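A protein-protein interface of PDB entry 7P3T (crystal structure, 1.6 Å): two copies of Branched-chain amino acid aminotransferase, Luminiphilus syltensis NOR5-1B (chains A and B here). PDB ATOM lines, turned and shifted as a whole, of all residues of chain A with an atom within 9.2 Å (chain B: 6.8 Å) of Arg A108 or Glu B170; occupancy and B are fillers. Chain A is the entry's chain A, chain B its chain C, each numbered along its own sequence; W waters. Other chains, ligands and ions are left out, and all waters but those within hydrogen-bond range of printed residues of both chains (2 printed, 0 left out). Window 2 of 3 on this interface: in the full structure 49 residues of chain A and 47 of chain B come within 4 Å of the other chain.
The guanidinium group (NH1) of Arg A97 lies within hydrogen-bond range of the backbone carbonyl oxygen (O) of Arg A63 (3.0 Å). The guanidinium group of Arg A97 is in hydrogen-bond range of the backbone carbonyl oxygen of Pro A107 (3.0 Å). OD2 of Asp A106 is in salt-bridge range of NH2 of Arg A108, 2.9 Å away.
Arg A63 touches Leu B166 (CD to CD2, 3.0 Å). Arg B165 touches Val A104. Leu B169 touches Asp A106 (CD1 to OD1, 3.5 Å). Pro A107 touches Leu B166 (CG to N, 3.9 Å). CD of Pro A107 touches CD1 of Leu B169, 3.9 Å away. Leu B166 touches Arg A108. Arg A108 touches Leu B169 (NH2 to CB, 3.7 Å).
The guanidinium group of Arg A63 lies within salt-bridge range of the side-chain carboxylate of Glu B170. The guanidinium group of Arg B165 is in hydrogen-bond range of the backbone carbonyl oxygen of Ala A105. OE2 of Glu B170 is in salt-bridge range of NH1 of Arg A108, at 2.9 Å.
No position is printed for both chains. Of the 10 pairs that touch across the chains among the printed residues, none has its exchanged pair printed and touching as well.
Of the 9 printed residues of chain B, 4 touch a printed residue of chain A. Of the 17 printed residues of chain A, 6 touch a printed residue of chain B. Hydrophobic or aromatic side chains of chain A within 4 Å of the printed part of chain B: Val A104 and Pro A107. Among the printed residues, Asp or Glu carboxylates within 4 Å of a Lys or Arg side-chain nitrogen of the other chain: Arg A63 with Glu B170 and Arg A108 with Glu B170.
Water W1 bridges the side-chain carboxylate (OE2) of Glu B170 (2.5 Å) and the guanidinium group (NH2) of Arg A63 (3.2 Å). Water W2 bridges the guanidinium group (NE) of Arg B165 (3.2 Å) and the backbone carbonyl oxygen (O) of Ala A105 (3.3 Å).
Gln A26 touches none of the printed residues of chain B. Printed residues of chain B within 4 Å of Val A104: Arg B165 (3.9 Å). Arg A108 touches just these residues of chain B: Leu B166 (3.4 Å), Leu B169 (3.7 Å) and Glu B170 (2.9 Å). Lys A111 touches none of the printed residues of chain B. Printed residues of chain A within 4 Å of Arg B165: Val A104 (3.9 Å) and Ala A105 (3.0 Å). Of the printed residues of chain A, Leu B166 touches Arg A63 (3.0 Å), Pro A107 (3.9 Å) and Arg A108 (3.4 Å). Leu B169 touches three residues of chain A. No residue of chain A comes within 4 Å of Ala B171. The nearest residue of chain B that does not touch Arg A108 is Ala B171 (6.3 Å). The nearest printed residue of chain A that does not touch Glu B170 is Asp A106 (6.8 Å). The nearest printed residue of chain B that does not touch Arg A63 is Glu B167 (6.8 Å).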
ATOM      1  N   GLN A  26     -14.515   5.690 -19.145  1.00  0.00           N
ATOM      2  CA  GLN A  26     -15.119   6.976 -18.770  1.00  0.00           C
ATOM      3  C   GLN A  26     -15.062   7.236 -17.272  1.00  0.00           C
ATOM      4  O   GLN A  26     -15.190   8.397 -16.840  1.00  0.00           O
ATOM      5  CB  GLN A  26     -16.558   7.023 -19.285  1.00  0.00           C
ATOM      6  CG  GLN A  26     -16.623   7.119 -20.797  1.00  0.00           C
ATOM      7  CD  GLN A  26     -18.004   6.877 -21.360  1.00  0.00           C
ATOM      8  OE1 GLN A  26     -18.656   7.813 -21.829  1.00  0.00           O
ATOM      9  NE2 GLN A  26     -18.446   5.613 -21.358  1.00  0.00           N
ATOM     10  N   ASP A  32     -16.821   9.316 -14.410  1.00  0.00           N
ATOM     11  CA  ASP A  32     -18.195   8.844 -14.580  1.00  0.00           C
ATOM     12  C   ASP A  32     -18.329   7.491 -13.890  1.00  0.00           C
ATOM     13  O   ASP A  32     -18.337   6.418 -14.505  1.00  0.00           O
ATOM     14  CB  ASP A  32     -18.559   8.803 -16.057  1.00  0.00           C
ATOM     15  CG  ASP A  32     -20.040   8.645 -16.288  1.00  0.00           C
ATOM     16  OD1 ASP A  32     -20.774   8.426 -15.298  1.00  0.00           O
ATOM     17  OD2 ASP A  32     -20.463   8.730 -17.458  1.00  0.00           O
ATOM     18  N   ALA A  62     -27.344   8.480 -10.857  1.00  0.00           N
ATOM     19  CA  ALA A  62     -26.425   8.718 -11.965  1.00  0.00           C
ATOM     20  C   ALA A  62     -26.788   7.911 -13.213  1.00  0.00           C
ATOM     21  O   ALA A  62     -26.017   7.907 -14.182  1.00  0.00           O
ATOM     22  CB  ALA A  62     -24.997   8.397 -11.519  1.00  0.00           C
ATOM     23  N   ARG A  63     -27.938   7.235 -13.206  1.00  0.00           N
ATOM     24  CA  ARG A  63     -28.386   6.409 -14.339  1.00  0.00           C
ATOM     25  C   ARG A  63     -27.308   5.399 -14.747  1.00  0.00           C
ATOM     26  O   ARG A  63     -27.089   5.123 -15.933  1.00  0.00           O
ATOM     27  CB  ARG A  63     -28.815   7.289 -15.517  1.00  0.00           C
ATOM     28  CG  ARG A  63     -30.118   8.068 -15.287  1.00  0.00           C
ATOM     29  CD  ARG A  63     -30.877   8.350 -16.596  1.00  0.00           C
ATOM     30  NE  ARG A  63     -31.201   7.135 -17.342  1.00  0.00           N
ATOM     31  CZ  ARG A  63     -31.898   7.115 -18.479  1.00  0.00           C
ATOM     32  NH1 ARG A  63     -32.345   8.243 -19.000  1.00  0.00           N
ATOM     33  NH2 ARG A  63     -32.145   5.968 -19.099  1.00  0.00           N
ATOM     34  N   LEU A  64     -26.650   4.808 -13.750  1.00  0.00           N
ATOM     35  CA  LEU A  64     -25.660   3.760 -13.978  1.00  0.00           C
ATOM     36  C   LEU A  64     -26.261   2.369 -13.834  1.00  0.00           C
ATOM     37  O   LEU A  64     -25.518   1.380 -13.736  1.00  0.00           O
ATOM     38  CB  LEU A  64     -24.471   3.941 -13.042  1.00  0.00           C
ATOM     39  CG  LEU A  64     -23.510   5.033 -13.528  1.00  0.00           C
ATOM     40  CD1 LEU A  64     -22.527   5.463 -12.421  1.00  0.00           C
ATOM     41  CD2 LEU A  64     -22.698   4.573 -14.745  1.00  0.00           C
ATOM     42  N   ASN A  65     -27.584   2.272 -13.885  1.00  0.00           N
ATOM     43  CA  ASN A  65     -28.243   0.986 -13.751  1.00  0.00           C
ATOM     44  C   ASN A  65     -27.701   0.033 -14.810  1.00  0.00           C
ATOM     45  O   ASN A  65     -27.545   0.400 -15.978  1.00  0.00           O
ATOM     46  CB  ASN A  65     -29.754   1.157 -13.880  1.00  0.00           C
ATOM     47  CG  ASN A  65     -30.283   2.311 -13.032  1.00  0.00           C
ATOM     48  OD1 ASN A  65     -30.066   3.473 -13.367  1.00  0.00           O
ATOM     49  ND2 ASN A  65     -30.944   1.995 -11.911  1.00  0.00           N
ATOM     50  N   HIS A  66     -27.394  -1.195 -14.394  1.00  0.00           N
ATOM     51  CA  HIS A  66     -26.686  -2.143 -15.245  1.00  0.00           C
ATOM     52  C   HIS A  66     -27.183  -3.541 -14.874  1.00  0.00           C
ATOM     53  O   HIS A  66     -28.125  -3.699 -14.091  1.00  0.00           O
ATOM     54  CB  HIS A  66     -25.168  -1.948 -15.120  1.00  0.00           C
ATOM     55  CG  HIS A  66     -24.642  -2.122 -13.727  1.00  0.00           C
ATOM     56  ND1 HIS A  66     -24.769  -1.157 -12.748  1.00  0.00           N
ATOM     57  CD2 HIS A  66     -24.001  -3.163 -13.143  1.00  0.00           C
ATOM     58  CE1 HIS A  66     -24.242  -1.601 -11.622  1.00  0.00           C
ATOM     59  NE2 HIS A  66     -23.749  -2.807 -11.842  1.00  0.00           N
ATOM     60  N   ARG A  97     -19.178   4.042 -15.992  1.00  0.00           N
ATOM     61  CA  ARG A  97     -19.845   3.991 -17.302  1.00  0.00           C
ATOM     62  C   ARG A  97     -19.033   3.214 -18.338  1.00  0.00           C
ATOM     63  O   ARG A  97     -19.522   2.960 -19.448  1.00  0.00           O
ATOM     64  CB  ARG A  97     -20.131   5.422 -17.790  1.00  0.00           C
ATOM     65  CG  ARG A  97     -21.075   5.582 -18.992  1.00  0.00           C
ATOM     66  CD  ARG A  97     -22.477   6.105 -18.706  1.00  0.00           C
ATOM     67  NE  ARG A  97     -22.554   7.044 -17.596  1.00  0.00           N
ATOM     68  CZ  ARG A  97     -23.629   7.191 -16.834  1.00  0.00           C
ATOM     69  NH1 ARG A  97     -24.727   6.502 -17.097  1.00  0.00           N
ATOM     70  NH2 ARG A  97     -23.595   8.021 -15.802  1.00  0.00           N
ATOM     71  N   LYS A 101     -19.028   2.845 -26.001  1.00  0.00           N
ATOM     72  CA  LYS A 101     -19.853   1.847 -26.667  1.00  0.00           C
ATOM     73  C   LYS A 101     -20.615   2.555 -27.774  1.00  0.00           C
ATOM     74  O   LYS A 101     -21.241   3.592 -27.535  1.00  0.00           O
ATOM     75  CB  LYS A 101     -20.820   1.192 -25.679  1.00  0.00           C
ATOM     76  CG  LYS A 101     -21.820   0.236 -26.301  1.00  0.00           C
ATOM     77  CD  LYS A 101     -22.737  -0.333 -25.212  1.00  0.00           C
ATOM     78  CE  LYS A 101     -23.585  -1.486 -25.723  1.00  0.00           C
ATOM     79  NZ  LYS A 101     -24.550  -1.044 -26.767  1.00  0.00           N
ATOM     80  N   VAL A 104     -21.249   7.314 -31.090  1.00  0.00           N
ATOM     81  CA  VAL A 104     -21.674   8.464 -30.316  1.00  0.00           C
ATOM     82  C   VAL A 104     -21.842   7.994 -28.878  1.00  0.00           C
ATOM     83  O   VAL A 104     -22.604   7.061 -28.609  1.00  0.00           O
ATOM     84  CB  VAL A 104     -22.978   9.047 -30.879  1.00  0.00           C
ATOM     85  CG1 VAL A 104     -24.063   7.975 -30.925  1.00  0.00           C
ATOM     86  CG2 VAL A 104     -23.429  10.244 -30.061  1.00  0.00           C
ATOM     87  N   ALA A 105     -21.100   8.607 -27.960  1.00  0.00           N
ATOM     88  CA  ALA A 105     -21.236   8.269 -26.550  1.00  0.00           C
ATOM     89  C   ALA A 105     -22.561   8.818 -26.027  1.00  0.00           C
ATOM     90  O   ALA A 105     -22.816  10.026 -26.096  1.00  0.00           O
ATOM     91  CB  ALA A 105     -20.057   8.818 -25.751  1.00  0.00           C
ATOM     92  N   ASP A 106     -23.404   7.918 -25.532  1.00  0.00           N
ATOM     93  CA  ASP A 106     -24.726   8.234 -24.988  1.00  0.00           C
ATOM     94  C   ASP A 106     -24.734   7.596 -23.608  1.00  0.00           C
ATOM     95  O   ASP A 106     -24.681   6.355 -23.507  1.00  0.00           O
ATOM     96  CB  ASP A 106     -25.820   7.685 -25.904  1.00  0.00           C
ATOM     97  CG  ASP A 106     -27.235   7.863 -25.352  1.00  0.00           C
ATOM     98  OD1 ASP A 106     -27.401   8.120 -24.161  1.00  0.00           O
ATOM     99  OD2 ASP A 106     -28.192   7.726 -26.136  1.00  0.00           O
ATOM    100  N   PRO A 107     -24.753   8.375 -22.523  1.00  0.00           N
ATOM    101  CA  PRO A 107     -24.642   7.759 -21.188  1.00  0.00           C
ATOM    102  C   PRO A 107     -25.753   6.766 -20.860  1.00  0.00           C
ATOM    103  O   PRO A 107     -25.632   6.040 -19.875  1.00  0.00           O
ATOM    104  CB  PRO A 107     -24.661   8.963 -20.227  1.00  0.00           C
ATOM    105  CG  PRO A 107     -25.084  10.137 -21.043  1.00  0.00           C
ATOM    106  CD  PRO A 107     -24.744   9.851 -22.459  1.00  0.00           C
ATOM    107  N   ARG A 108     -26.813   6.677 -21.657  1.00  0.00           N
ATOM    108  CA  ARG A 108     -27.853   5.687 -21.405  1.00  0.00           C
ATOM    109  C   ARG A 108     -27.518   4.319 -21.977  1.00  0.00           C
ATOM    110  O   ARG A 108     -28.192   3.333 -21.652  1.00  0.00           O
ATOM    111  CB  ARG A 108     -29.172   6.214 -21.971  1.00  0.00           C
ATOM    112  CG  ARG A 108     -29.482   7.623 -21.502  1.00  0.00           C
ATOM    113  CD  ARG A 108     -30.644   8.207 -22.258  1.00  0.00           C
ATOM    114  NE  ARG A 108     -30.292   8.433 -23.653  1.00  0.00           N
ATOM    115  CZ  ARG A 108     -31.107   8.953 -24.563  1.00  0.00           C
ATOM    116  NH1 ARG A 108     -32.341   9.308 -24.230  1.00  0.00           N
ATOM    117  NH2 ARG A 108     -30.692   9.103 -25.815  1.00  0.00           N
ATOM    118  N   ASP A 109     -26.484   4.221 -22.798  1.00  0.00           N
ATOM    119  CA  ASP A 109     -26.133   2.983 -23.486  1.00  0.00           C
ATOM    120  C   ASP A 109     -24.664   2.701 -23.183  1.00  0.00           C
ATOM    121  O   ASP A 109     -23.780   3.372 -23.725  1.00  0.00           O
ATOM    122  CB  ASP A 109     -26.396   3.132 -24.975  1.00  0.00           C
ATOM    123  CG  ASP A 109     -26.155   1.864 -25.732  1.00  0.00           C
ATOM    124  OD1 ASP A 109     -26.181   0.790 -25.104  1.00  0.00           O
ATOM    125  OD2 ASP A 109     -25.944   1.945 -26.957  1.00  0.00           O
ATOM    126  N   PHE A 110     -24.403   1.740 -22.295  1.00  0.00           N
ATOM    127  CA  PHE A 110     -23.037   1.533 -21.837  1.00  0.00           C
ATOM    128  C   PHE A 110     -22.847   0.118 -21.308  1.00  0.00           C
ATOM    129  O   PHE A 110     -23.806  -0.590 -20.983  1.00  0.00           O
ATOM    130  CB  PHE A 110     -22.674   2.563 -20.750  1.00  0.00           C
ATOM    131  CG  PHE A 110     -23.413   2.365 -19.469  1.00  0.00           C
ATOM    132  CD1 PHE A 110     -24.687   2.865 -19.301  1.00  0.00           C
ATOM    133  CD2 PHE A 110     -22.833   1.663 -18.424  1.00  0.00           C
ATOM    134  CE1 PHE A 110     -25.376   2.658 -18.120  1.00  0.00           C
ATOM    135  CE2 PHE A 110     -23.521   1.481 -17.233  1.00  0.00           C
ATOM    136  CZ  PHE A 110     -24.783   1.958 -17.095  1.00  0.00           C
ATOM    137  N   LYS A 111     -21.575  -0.290 -21.288  1.00  0.00           N
ATOM    138  CA  LYS A 111     -21.108  -1.527 -20.682  1.00  0.00           C
ATOM    139  C   LYS A 111     -20.285  -1.145 -19.464  1.00  0.00           C
ATOM    140  O   LYS A 111     -19.217  -0.536 -19.622  1.00  0.00           O
ATOM    141  CB  LYS A 111     -20.257  -2.330 -21.665  1.00  0.00           C
ATOM    142  CG  LYS A 111     -20.003  -3.746 -21.214  1.00  0.00           C
ATOM    143  CD  LYS A 111     -18.762  -4.338 -21.875  1.00  0.00           C
ATOM    144  CE  LYS A 111     -18.403  -5.678 -21.242  1.00  0.00           C
ATOM    145  NZ  LYS A 111     -17.191  -5.599 -20.374  1.00  0.00           N
ATOM    146  N   ARG B 165     -25.499  15.798 -19.931  1.00  0.00           N
ATOM    147  CA  ARG B 165     -25.677  15.205 -21.250  1.00  0.00           C
ATOM    148  C   ARG B 165     -26.857  14.258 -21.278  1.00  0.00           C
ATOM    149  O   ARG B 165     -27.611  14.218 -22.260  1.00  0.00           O
ATOM    150  CB  ARG B 165     -24.403  14.471 -21.650  1.00  0.00           C
ATOM    151  CG  ARG B 165     -24.472  13.832 -22.977  1.00  0.00           C
ATOM    152  CD  ARG B 165     -23.067  13.649 -23.568  1.00  0.00           C
ATOM    153  NE  ARG B 165     -23.184  12.920 -24.826  1.00  0.00           N
ATOM    154  CZ  ARG B 165     -23.837  13.371 -25.894  1.00  0.00           C
ATOM    155  NH1 ARG B 165     -24.389  14.578 -25.892  1.00  0.00           N
ATOM    156  NH2 ARG B 165     -23.918  12.618 -26.980  1.00  0.00           N
ATOM    157  N   LEU B 166     -27.009  13.466 -20.223  1.00  0.00           N
ATOM    158  CA  LEU B 166     -28.158  12.532 -20.161  1.00  0.00           C
ATOM    159  C   LEU B 166     -29.466  13.332 -20.239  1.00  0.00           C
ATOM    160  O   LEU B 166     -30.348  12.936 -20.953  1.00  0.00           O
ATOM    161  CB  LEU B 166     -28.130  11.757 -18.849  1.00  0.00           C
ATOM    162  CG  LEU B 166     -29.512  11.286 -18.407  1.00  0.00           C
ATOM    163  CD1 LEU B 166     -29.944  10.072 -19.195  1.00  0.00           C
ATOM    164  CD2 LEU B 166     -29.593  11.018 -16.917  1.00  0.00           C
ATOM    165  N   GLU B 167     -29.547  14.421 -19.486  1.00  0.00           N
ATOM    166  CA  GLU B 167     -30.747  15.256 -19.469  1.00  0.00           C
ATOM    167  C   GLU B 167     -30.985  15.908 -20.821  1.00  0.00           C
ATOM    168  O   GLU B 167     -32.124  15.959 -21.294  1.00  0.00           O
ATOM    169  CB  GLU B 167     -30.634  16.303 -18.373  1.00  0.00           C
ATOM    170  CG  GLU B 167     -30.934  15.698 -17.015  1.00  0.00           C
ATOM    171  CD  GLU B 167     -30.322  16.457 -15.866  1.00  0.00           C
ATOM    172  OE1 GLU B 167     -29.953  17.640 -16.042  1.00  0.00           O
ATOM    173  OE2 GLU B 167     -30.229  15.863 -14.771  1.00  0.00           O
ATOM    174  N   ALA B 168     -29.924  16.372 -21.475  1.00  0.00           N
ATOM    175  CA  ALA B 168     -30.093  16.978 -22.791  1.00  0.00           C
ATOM    176  C   ALA B 168     -30.640  15.968 -23.791  1.00  0.00           C
ATOM    177  O   ALA B 168     -31.543  16.273 -24.581  1.00  0.00           O
ATOM    178  CB  ALA B 168     -28.758  17.537 -23.274  1.00  0.00           C
ATOM    179  N   LEU B 169     -30.108  14.746 -23.774  1.00  0.00           N
ATOM    180  CA  LEU B 169     -30.587  13.736 -24.708  1.00  0.00           C
ATOM    181  C   LEU B 169     -32.030  13.361 -24.415  1.00  0.00           C
ATOM    182  O   LEU B 169     -32.838  13.227 -25.340  1.00  0.00           O
ATOM    183  CB  LEU B 169     -29.682  12.506 -24.667  1.00  0.00           C
ATOM    184  CG  LEU B 169     -28.248  12.783 -25.118  1.00  0.00           C
ATOM    185  CD1 LEU B 169     -27.366  11.570 -24.825  1.00  0.00           C
ATOM    186  CD2 LEU B 169     -28.198  13.126 -26.607  1.00  0.00           C
ATOM    187  N   GLU B 170     -32.386  13.203 -23.136  1.00  0.00           N
ATOM    188  CA  GLU B 170     -33.766  12.866 -22.813  1.00  0.00           C
ATOM    189  C   GLU B 170     -34.725  13.954 -23.276  1.00  0.00           C
ATOM    190  O   GLU B 170     -35.887  13.662 -23.606  1.00  0.00           O
ATOM    191  CB  GLU B 170     -33.938  12.679 -21.306  1.00  0.00           C
ATOM    192  CG  GLU B 170     -33.433  11.381 -20.763  1.00  0.00           C
ATOM    193  CD  GLU B 170     -34.242  10.195 -21.240  1.00  0.00           C
ATOM    194  OE1 GLU B 170     -35.491  10.246 -21.239  1.00  0.00           O
ATOM    195  OE2 GLU B 170     -33.614   9.216 -21.624  1.00  0.00           O
ATOM    196  N   ALA B 171     -34.269  15.195 -23.280  1.00  0.00           N
ATOM    197  CA  ALA B 171     -35.097  16.342 -23.639  1.00  0.00           C
ATOM    198  C   ALA B 171     -35.104  16.603 -25.135  1.00  0.00           C
ATOM    199  O   ALA B 171     -35.791  17.521 -25.587  1.00  0.00           O
ATOM    200  CB  ALA B 171     -34.609  17.604 -22.925  1.00  0.00           C
ATOM    201  N   GLY B 172     -34.317  15.858 -25.903  1.00  0.00           N
ATOM    202  CA  GLY B 172     -34.343  15.989 -27.347  1.00  0.00           C
ATOM    203  C   GLY B 172     -33.463  17.084 -27.896  1.00  0.00           C
ATOM    204  O   GLY B 172     -33.675  17.516 -29.035  1.00  0.00           O
ATOM    205  N   TYR B 173     -32.467  17.530 -27.139  1.00  0.00           N
ATOM    206  CA  TYR B 173     -31.583  18.599 -27.564  1.00  0.00           C
ATOM    207  C   TYR B 173     -30.213  18.062 -27.943  1.00  0.00           C
ATOM    208  O   TYR B 173     -29.815  16.970 -27.542  1.00  0.00           O
ATOM    209  CB  TYR B 173     -31.439  19.627 -26.449  1.00  0.00           C
ATOM    210  CG  TYR B 173     -32.620  20.560 -26.289  1.00  0.00           C
ATOM    211  CD1 TYR B 173     -32.701  21.741 -27.026  1.00  0.00           C
ATOM    212  CD2 TYR B 173     -33.671  20.249 -25.423  1.00  0.00           C
ATOM    213  CE1 TYR B 173     -33.779  22.604 -26.872  1.00  0.00           C
ATOM    214  CE2 TYR B 173     -34.752  21.106 -25.268  1.00  0.00           C
ATOM    215  CZ  TYR B 173     -34.798  22.282 -25.990  1.00  0.00           C
ATOM    216  OH  TYR B 173     -35.882  23.112 -25.820  1.00  0.00           O
HETATM  217  O   HOH W   1     -34.070   6.805 -21.530  1.00  0.00           O
HETATM  218  O   HOH W   2     -21.475  10.794 -23.173  1.00  0.00           O
